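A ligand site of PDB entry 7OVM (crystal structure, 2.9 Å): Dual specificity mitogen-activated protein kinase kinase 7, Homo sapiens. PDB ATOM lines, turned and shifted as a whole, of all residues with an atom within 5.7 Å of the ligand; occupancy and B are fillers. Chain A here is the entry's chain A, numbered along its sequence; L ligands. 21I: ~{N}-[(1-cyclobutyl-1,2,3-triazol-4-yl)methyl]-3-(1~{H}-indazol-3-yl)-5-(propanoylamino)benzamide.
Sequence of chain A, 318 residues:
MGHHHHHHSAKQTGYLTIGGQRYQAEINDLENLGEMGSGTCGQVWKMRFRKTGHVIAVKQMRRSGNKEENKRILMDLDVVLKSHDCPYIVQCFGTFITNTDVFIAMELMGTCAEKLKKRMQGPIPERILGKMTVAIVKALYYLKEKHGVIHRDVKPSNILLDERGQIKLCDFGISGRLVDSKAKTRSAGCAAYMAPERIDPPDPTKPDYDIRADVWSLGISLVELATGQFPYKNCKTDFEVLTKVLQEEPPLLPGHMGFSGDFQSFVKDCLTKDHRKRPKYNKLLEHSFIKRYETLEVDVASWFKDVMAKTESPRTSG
The backbone NH of Lys 115 sits at hydrogen-bond distance from the side-chain sulfur of Cys 112 (3.5 Å). N of Met 36 is in hydrogen-bond range of O of Val 44. O of Ala 57 is in hydrogen-bond range of N of Met 106 (2.5 Å).
The backbone NH of Cys 112 sits close to an oxygen (OBG) of the ligand (3.3 Å). SG of Cys 112 is bonded to CAU of the ligand, 1.8 Å away. The backbone carbonyl oxygen (O) of Glu 107 is in hydrogen-bond range of a nitrogen (NAY) of the ligand. The backbone NH of Met 109 is in hydrogen-bond range of a nitrogen (NAZ) of the ligand (2.9 Å). A nitrogen (NAR) of the ligand sits close to the backbone carbonyl oxygen (O) of Met 109 (3.5 Å). O of Gly 37 is in hydrogen-bond range of NBD of the ligand, 3.1 Å away. The side-chain sulfur of Met 36 sits at hydrogen-bond distance from a nitrogen (NAR) of the ligand (3.2 Å).
O of Gly 110 lies close to OAS of the ligand. Residues that only touch the ligand: Ser 38 (3.8 Å), Lys 46 (3.6 Å), Val 90 (3.6 Å), Met 106 (3.9 Å), Leu 108 (3.4 Å), Thr 111 (3.6 Å), Ser 157 (3.5 Å) and Leu 160 (3.4 Å). Hydrophobic or aromatic side chains that line the ligand: Met 36, Val 90, Met 106, Leu 108, Met 109 and Leu 160. 14 residues have an atom within 4 Å of the ligand: Met 36, Gly 37, Ser 38, Lys 46, Val 90, Met 106, Glu 107, Leu 108, Met 109, Gly 110, Thr 111, Cys 112, Ser 157 and Leu 160. The nearest printed residue that does not touch the ligand is Ala 57 (4.1 Å).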
ATOM      1  N   MET A  36      -6.180 -21.682  -0.937  1.00  0.00           N
ATOM      2  CA  MET A  36      -5.114 -22.028  -1.864  1.00  0.00           C
ATOM      3  C   MET A  36      -3.826 -22.318  -1.092  1.00  0.00           C
ATOM      4  O   MET A  36      -3.591 -21.742  -0.021  1.00  0.00           O
ATOM      5  CB  MET A  36      -4.866 -20.900  -2.882  1.00  0.00           C
ATOM      6  CG  MET A  36      -6.121 -20.474  -3.631  1.00  0.00           C
ATOM      7  SD  MET A  36      -5.792 -19.246  -4.906  1.00  0.00           S
ATOM      8  CE  MET A  36      -5.003 -17.967  -3.937  1.00  0.00           C
ATOM      9  N   GLY A  37      -3.015 -23.207  -1.642  1.00  0.00           N
ATOM     10  CA  GLY A  37      -1.787 -23.615  -0.987  1.00  0.00           C
ATOM     11  C   GLY A  37      -0.597 -22.762  -1.348  1.00  0.00           C
ATOM     12  O   GLY A  37      -0.134 -22.767  -2.496  1.00  0.00           O
ATOM     13  N   SER A  38      -0.062 -22.032  -0.376  1.00  0.00           N
ATOM     14  CA  SER A  38       1.102 -21.181  -0.581  1.00  0.00           C
ATOM     15  C   SER A  38       1.740 -20.896   0.772  1.00  0.00           C
ATOM     16  O   SER A  38       1.186 -21.225   1.819  1.00  0.00           O
ATOM     17  CB  SER A  38       0.731 -19.886  -1.300  1.00  0.00           C
ATOM     18  OG  SER A  38      -0.120 -19.079  -0.496  1.00  0.00           O
ATOM     19  N   GLY A  39       2.918 -20.279   0.720  1.00  0.00           N
ATOM     20  CA  GLY A  39       3.613 -19.885   1.929  1.00  0.00           C
ATOM     21  C   GLY A  39       2.850 -18.827   2.712  1.00  0.00           C
ATOM     22  O   GLY A  39       2.687 -17.697   2.235  1.00  0.00           O
ATOM     23  N   VAL A  44      -4.670 -17.372   2.379  1.00  0.00           N
ATOM     24  CA  VAL A  44      -5.129 -16.795   1.126  1.00  0.00           C
ATOM     25  C   VAL A  44      -6.287 -17.630   0.587  1.00  0.00           C
ATOM     26  O   VAL A  44      -6.193 -18.860   0.511  1.00  0.00           O
ATOM     27  CB  VAL A  44      -3.988 -16.716   0.095  1.00  0.00           C
ATOM     28  CG1 VAL A  44      -4.382 -15.833  -1.070  1.00  0.00           C
ATOM     29  CG2 VAL A  44      -2.711 -16.200   0.756  1.00  0.00           C
ATOM     30  N   LYS A  46      -9.293 -18.202  -2.568  1.00  0.00           N
ATOM     31  CA  LYS A  46      -9.686 -17.962  -3.952  1.00  0.00           C
ATOM     32  C   LYS A  46     -11.175 -17.613  -3.961  1.00  0.00           C
ATOM     33  O   LYS A  46     -12.008 -18.444  -3.582  1.00  0.00           O
ATOM     34  CB  LYS A  46      -9.411 -19.190  -4.826  1.00  0.00           C
ATOM     35  CG  LYS A  46      -9.856 -19.025  -6.268  1.00  0.00           C
ATOM     36  CD  LYS A  46      -9.271 -20.126  -7.153  1.00  0.00           C
ATOM     37  CE  LYS A  46      -9.649 -21.510  -6.656  1.00  0.00           C
ATOM     38  NZ  LYS A  46      -9.055 -22.581  -7.493  1.00  0.00           N
ATOM     39  N   VAL A  55     -12.382 -13.968 -10.750  1.00  0.00           N
ATOM     40  CA  VAL A  55     -11.782 -14.820  -9.727  1.00  0.00           C
ATOM     41  C   VAL A  55     -10.531 -14.128  -9.201  1.00  0.00           C
ATOM     42  O   VAL A  55      -9.606 -13.845  -9.970  1.00  0.00           O
ATOM     43  CB  VAL A  55     -11.467 -16.211 -10.278  1.00  0.00           C
ATOM     44  CG1 VAL A  55     -10.746 -17.047  -9.237  1.00  0.00           C
ATOM     45  CG2 VAL A  55     -12.739 -16.904 -10.736  1.00  0.00           C
ATOM     46  N   ALA A  57      -7.681 -13.493  -5.656  1.00  0.00           N
ATOM     47  CA  ALA A  57      -7.046 -14.068  -4.479  1.00  0.00           C
ATOM     48  C   ALA A  57      -7.231 -13.111  -3.308  1.00  0.00           C
ATOM     49  O   ALA A  57      -6.863 -11.935  -3.405  1.00  0.00           O
ATOM     50  CB  ALA A  57      -5.561 -14.336  -4.736  1.00  0.00           C
ATOM     51  N   LYS A  59      -6.428 -12.794   0.699  1.00  0.00           N
ATOM     52  CA  LYS A  59      -5.789 -13.250   1.928  1.00  0.00           C
ATOM     53  C   LYS A  59      -6.446 -12.582   3.124  1.00  0.00           C
ATOM     54  O   LYS A  59      -6.615 -11.355   3.149  1.00  0.00           O
ATOM     55  CB  LYS A  59      -4.289 -12.977   1.904  1.00  0.00           C
ATOM     56  CG  LYS A  59      -3.909 -11.552   1.507  1.00  0.00           C
ATOM     57  CD  LYS A  59      -2.427 -11.305   1.701  1.00  0.00           C
ATOM     58  CE  LYS A  59      -1.578 -12.274   0.892  1.00  0.00           C
ATOM     59  NZ  LYS A  59      -0.117 -12.044   1.097  1.00  0.00           N
ATOM     60  N   VAL A  90       2.923  -8.583  -7.890  1.00  0.00           N
ATOM     61  CA  VAL A  90       1.522  -8.964  -7.728  1.00  0.00           C
ATOM     62  C   VAL A  90       0.741  -7.771  -7.199  1.00  0.00           C
ATOM     63  O   VAL A  90       1.138  -7.127  -6.227  1.00  0.00           O
ATOM     64  CB  VAL A  90       1.397 -10.190  -6.811  1.00  0.00           C
ATOM     65  CG1 VAL A  90       2.086  -9.955  -5.474  1.00  0.00           C
ATOM     66  CG2 VAL A  90      -0.072 -10.556  -6.607  1.00  0.00           C
ATOM     67  N   MET A 106      -5.757  -9.711  -3.727  1.00  0.00           N
ATOM     68  CA  MET A 106      -4.672  -9.807  -4.689  1.00  0.00           C
ATOM     69  C   MET A 106      -5.186 -10.398  -5.997  1.00  0.00           C
ATOM     70  O   MET A 106      -6.218 -11.068  -6.047  1.00  0.00           O
ATOM     71  CB  MET A 106      -3.533 -10.665  -4.151  1.00  0.00           C
ATOM     72  CG  MET A 106      -2.847 -10.095  -2.910  1.00  0.00           C
ATOM     73  SD  MET A 106      -1.981  -8.555  -3.247  1.00  0.00           S
ATOM     74  CE  MET A 106      -1.186  -8.257  -1.665  1.00  0.00           C
ATOM     75  N   GLU A 107      -4.449 -10.132  -7.080  1.00  0.00           N
ATOM     76  CA  GLU A 107      -4.802 -10.719  -8.359  1.00  0.00           C
ATOM     77  C   GLU A 107      -4.551 -12.225  -8.339  1.00  0.00           C
ATOM     78  O   GLU A 107      -3.683 -12.723  -7.621  1.00  0.00           O
ATOM     79  CB  GLU A 107      -4.009 -10.066  -9.487  1.00  0.00           C
ATOM     80  CG  GLU A 107      -2.507 -10.249  -9.399  1.00  0.00           C
ATOM     81  CD  GLU A 107      -1.777  -9.625 -10.570  1.00  0.00           C
ATOM     82  OE1 GLU A 107      -2.353  -9.584 -11.679  1.00  0.00           O
ATOM     83  OE2 GLU A 107      -0.634  -9.157 -10.373  1.00  0.00           O
ATOM     84  N   LEU A 108      -5.330 -12.949  -9.136  1.00  0.00           N
ATOM     85  CA  LEU A 108      -5.265 -14.396  -9.171  1.00  0.00           C
ATOM     86  C   LEU A 108      -4.317 -14.846 -10.269  1.00  0.00           C
ATOM     87  O   LEU A 108      -4.457 -14.435 -11.425  1.00  0.00           O
ATOM     88  CB  LEU A 108      -6.667 -14.989  -9.386  1.00  0.00           C
ATOM     89  CG  LEU A 108      -6.901 -16.459  -9.024  1.00  0.00           C
ATOM     90  CD1 LEU A 108      -6.490 -17.381 -10.157  1.00  0.00           C
ATOM     91  CD2 LEU A 108      -6.164 -16.822  -7.747  1.00  0.00           C
ATOM     92  N   MET A 109      -3.348 -15.674  -9.912  1.00  0.00           N
ATOM     93  CA  MET A 109      -2.369 -16.209 -10.843  1.00  0.00           C
ATOM     94  C   MET A 109      -2.390 -17.730 -10.796  1.00  0.00           C
ATOM     95  O   MET A 109      -3.019 -18.350  -9.933  1.00  0.00           O
ATOM     96  CB  MET A 109      -0.959 -15.680 -10.542  1.00  0.00           C
ATOM     97  CG  MET A 109      -0.917 -14.183 -10.271  1.00  0.00           C
ATOM     98  SD  MET A 109       0.496 -13.367 -11.034  1.00  0.00           S
ATOM     99  CE  MET A 109      -0.087 -13.161 -12.708  1.00  0.00           C
ATOM    100  N   GLY A 110      -1.688 -18.340 -11.744  1.00  0.00           N
ATOM    101  CA  GLY A 110      -1.681 -19.789 -11.889  1.00  0.00           C
ATOM    102  C   GLY A 110      -1.017 -20.531 -10.747  1.00  0.00           C
ATOM    103  O   GLY A 110      -1.681 -21.262 -10.011  1.00  0.00           O
ATOM    104  N   THR A 111       0.297 -20.364 -10.604  1.00  0.00           N
ATOM    105  CA  THR A 111       1.059 -21.063  -9.582  1.00  0.00           C
ATOM    106  C   THR A 111       2.388 -20.343  -9.400  1.00  0.00           C
ATOM    107  O   THR A 111       2.620 -19.272  -9.961  1.00  0.00           O
ATOM    108  CB  THR A 111       1.266 -22.536  -9.972  1.00  0.00           C
ATOM    109  OG1 THR A 111       2.018 -23.202  -8.944  1.00  0.00           O
ATOM    110  CG2 THR A 111       2.014 -22.640 -11.292  1.00  0.00           C
ATOM    111  N   CYS A 112       3.282 -20.944  -8.607  1.00  0.00           N
ATOM    112  CA  CYS A 112       4.620 -20.437  -8.389  1.00  0.00           C
ATOM    113  C   CYS A 112       5.635 -21.297  -9.126  1.00  0.00           C
ATOM    114  O   CYS A 112       5.320 -22.391  -9.616  1.00  0.00           O
ATOM    115  CB  CYS A 112       4.958 -20.376  -6.901  1.00  0.00           C
ATOM    116  SG  CYS A 112       4.815 -21.955  -6.032  1.00  0.00           S
ATOM    117  N   ALA A 113       6.869 -20.806  -9.188  1.00  0.00           N
ATOM    118  CA  ALA A 113       7.924 -21.543  -9.876  1.00  0.00           C
ATOM    119  C   ALA A 113       8.290 -22.823  -9.139  1.00  0.00           C
ATOM    120  O   ALA A 113       8.751 -23.782  -9.768  1.00  0.00           O
ATOM    121  CB  ALA A 113       9.160 -20.663 -10.057  1.00  0.00           C
ATOM    122  N   GLU A 114       8.079 -22.871  -7.822  1.00  0.00           N
ATOM    123  CA  GLU A 114       8.369 -24.079  -7.071  1.00  0.00           C
ATOM    124  C   GLU A 114       7.417 -25.204  -7.442  1.00  0.00           C
ATOM    125  O   GLU A 114       7.844 -26.318  -7.766  1.00  0.00           O
ATOM    126  CB  GLU A 114       8.315 -23.798  -5.573  1.00  0.00           C
ATOM    127  CG  GLU A 114       8.639 -25.006  -4.713  1.00  0.00           C
ATOM    128  CD  GLU A 114       8.378 -24.768  -3.233  1.00  0.00           C
ATOM    129  OE1 GLU A 114       7.714 -23.772  -2.904  1.00  0.00           O
ATOM    130  OE2 GLU A 114       8.859 -25.573  -2.411  1.00  0.00           O
ATOM    131  N   LYS A 115       6.110 -24.919  -7.409  1.00  0.00           N
ATOM    132  CA  LYS A 115       5.133 -25.932  -7.788  1.00  0.00           C
ATOM    133  C   LYS A 115       5.215 -26.275  -9.268  1.00  0.00           C
ATOM    134  O   LYS A 115       4.943 -27.421  -9.653  1.00  0.00           O
ATOM    135  CB  LYS A 115       3.717 -25.465  -7.425  1.00  0.00           C
ATOM    136  N   PRO A 156      12.144 -19.757  -5.786  1.00  0.00           N
ATOM    137  CA  PRO A 156      11.103 -20.107  -6.760  1.00  0.00           C
ATOM    138  C   PRO A 156       9.687 -20.007  -6.210  1.00  0.00           C
ATOM    139  O   PRO A 156       8.748 -19.786  -6.987  1.00  0.00           O
ATOM    140  CB  PRO A 156      11.451 -21.555  -7.133  1.00  0.00           C
ATOM    141  CG  PRO A 156      12.920 -21.639  -6.920  1.00  0.00           C
ATOM    142  CD  PRO A 156      13.213 -20.774  -5.730  1.00  0.00           C
ATOM    143  N   SER A 157       9.499 -20.171  -4.899  1.00  0.00           N
ATOM    144  CA  SER A 157       8.164 -20.074  -4.329  1.00  0.00           C
ATOM    145  C   SER A 157       7.590 -18.658  -4.380  1.00  0.00           C
ATOM    146  O   SER A 157       6.398 -18.486  -4.134  1.00  0.00           O
ATOM    147  CB  SER A 157       8.168 -20.565  -2.879  1.00  0.00           C
ATOM    148  OG  SER A 157       8.973 -19.733  -2.063  1.00  0.00           O
ATOM    149  N   ASN A 158       8.408 -17.659  -4.707  1.00  0.00           N
ATOM    150  CA  ASN A 158       7.962 -16.270  -4.779  1.00  0.00           C
ATOM    151  C   ASN A 158       7.920 -15.733  -6.206  1.00  0.00           C
ATOM    152  O   ASN A 158       7.987 -14.520  -6.407  1.00  0.00           O
ATOM    153  CB  ASN A 158       8.849 -15.385  -3.910  1.00  0.00           C
ATOM    154  CG  ASN A 158       8.713 -15.692  -2.429  1.00  0.00           C
ATOM    155  OD1 ASN A 158       7.649 -16.104  -1.965  1.00  0.00           O
ATOM    156  ND2 ASN A 158       9.800 -15.501  -1.683  1.00  0.00           N
ATOM    157  N   LEU A 160       5.495 -15.937  -9.445  1.00  0.00           N
ATOM    158  CA  LEU A 160       4.169 -16.351  -9.876  1.00  0.00           C
ATOM    159  C   LEU A 160       4.041 -16.313 -11.394  1.00  0.00           C
ATOM    160  O   LEU A 160       4.722 -15.526 -12.078  1.00  0.00           O
ATOM    161  CB  LEU A 160       3.092 -15.461  -9.252  1.00  0.00           C
ATOM    162  CG  LEU A 160       3.119 -15.317  -7.728  1.00  0.00           C
ATOM    163  CD1 LEU A 160       1.974 -14.435  -7.263  1.00  0.00           C
ATOM    164  CD2 LEU A 160       3.065 -16.685  -7.060  1.00  0.00           C
ATOM    165  N   GLU A 163      -2.039 -17.808 -16.841  1.00  0.00           N
ATOM    166  CA  GLU A 163      -2.348 -18.290 -18.182  1.00  0.00           C
ATOM    167  C   GLU A 163      -1.911 -17.320 -19.263  1.00  0.00           C
ATOM    168  O   GLU A 163      -1.560 -17.740 -20.371  1.00  0.00           O
ATOM    169  CB  GLU A 163      -3.851 -18.561 -18.306  1.00  0.00           C
ATOM    170  CG  GLU A 163      -4.404 -19.531 -17.275  1.00  0.00           C
ATOM    171  CD  GLU A 163      -5.909 -19.684 -17.383  1.00  0.00           C
ATOM    172  OE1 GLU A 163      -6.520 -19.022 -18.256  1.00  0.00           O
ATOM    173  OE2 GLU A 163      -6.489 -20.465 -16.601  1.00  0.00           O
ATOM    174  N   CYS A 170       6.186 -11.996  -5.673  1.00  0.00           N
ATOM    175  CA  CYS A 170       5.176 -12.409  -4.705  1.00  0.00           C
ATOM    176  C   CYS A 170       5.270 -11.449  -3.534  1.00  0.00           C
ATOM    177  O   CYS A 170       5.004 -10.256  -3.706  1.00  0.00           O
ATOM    178  CB  CYS A 170       5.328 -13.877  -4.354  1.00  0.00           C
ATOM    179  SG  CYS A 170       3.916 -14.752  -3.599  1.00  0.00           S
ATOM    180  N   ASP A 171       5.650 -11.923  -2.350  1.00  0.00           N
ATOM    181  CA  ASP A 171       5.421 -11.140  -1.160  1.00  0.00           C
ATOM    182  C   ASP A 171       6.629 -11.068  -0.232  1.00  0.00           C
ATOM    183  O   ASP A 171       7.267 -12.081   0.094  1.00  0.00           O
ATOM    184  CB  ASP A 171       4.185 -11.620  -0.421  1.00  0.00           C
ATOM    185  CG  ASP A 171       3.027 -10.676  -0.667  1.00  0.00           C
ATOM    186  OD1 ASP A 171       3.289  -9.459  -0.653  1.00  0.00           O
ATOM    187  OD2 ASP A 171       1.901 -11.126  -0.947  1.00  0.00           O
HETATM  188  CAA 21I L   1      -0.588 -13.692  -3.874  1.00  0.00           C
HETATM  189  CAB 21I L   1      -0.320 -14.944  -3.358  1.00  0.00           C
HETATM  190  CAC 21I L   1      -0.671 -16.060  -4.104  1.00  0.00           C
HETATM  191  CAD 21I L   1      -1.255 -15.933  -5.300  1.00  0.00           C
HETATM  192  CAE 21I L   1      -1.517 -14.715  -5.788  1.00  0.00           C
HETATM  193  CAF 21I L   1      -1.202 -13.612  -5.106  1.00  0.00           C
HETATM  194  CAG 21I L   1      -1.701 -16.812  -6.219  1.00  0.00           C
HETATM  195  CAH 21I L   1      -9.617 -20.438 -12.029  1.00  0.00           C
HETATM  196  CAI 21I L   1     -10.026 -19.448 -13.116  1.00  0.00           C
HETATM  197  CAJ 21I L   1      -8.672 -18.816 -12.803  1.00  0.00           C
HETATM  198  CAK 21I L   1      -8.236 -20.258 -12.621  1.00  0.00           C
HETATM  199  CAO 21I L   1      -7.340 -20.762 -10.349  1.00  0.00           C
HETATM  200  CAP 21I L   1      -6.136 -20.785  -9.781  1.00  0.00           C
HETATM  201  CAQ 21I L   1      -5.890 -21.147  -8.311  1.00  0.00           C
HETATM  202  CAT 21I L   1      -3.669 -21.054  -7.302  1.00  0.00           C
HETATM  203  CAU 21I L   1       4.174 -21.138  -4.541  1.00  0.00           C
HETATM  204  CAV 21I L   1      -2.656 -20.277  -6.734  1.00  0.00           C
HETATM  205  CAW 21I L   1      -2.679 -18.886  -6.765  1.00  0.00           C
HETATM  206  CAX 21I L   1      -1.655 -18.152  -6.168  1.00  0.00           C
HETATM  207  CBA 21I L   1      -1.599 -20.943  -6.113  1.00  0.00           C
HETATM  208  CBB 21I L   1      -0.565 -20.233  -5.532  1.00  0.00           C
HETATM  209  CBC 21I L   1      -0.605 -18.837  -5.560  1.00  0.00           C
HETATM  210  CBE 21I L   1       1.712 -20.580  -5.118  1.00  0.00           C
HETATM  211  CBF 21I L   1       2.689 -21.482  -4.358  1.00  0.00           C
HETATM  212  NAL 21I L   1      -5.204 -20.463 -10.662  1.00  0.00           N
HETATM  213  NAM 21I L   1      -5.845 -20.227 -11.825  1.00  0.00           N
HETATM  214  NAN 21I L   1      -7.157 -20.417 -11.614  1.00  0.00           N
HETATM  215  NAR 21I L   1      -4.746 -20.400  -7.741  1.00  0.00           N
HETATM  216  NAY 21I L   1      -2.110 -14.852  -6.977  1.00  0.00           N
HETATM  217  NAZ 21I L   1      -2.216 -16.161  -7.245  1.00  0.00           N
HETATM  218  NBD 21I L   1       0.420 -20.906  -4.936  1.00  0.00           N
HETATM  219  OAS 21I L   1      -3.552 -22.278  -7.354  1.00  0.00           O
HETATM  220  OBG 21I L   1       2.127 -19.663  -5.835  1.00  0.00           O
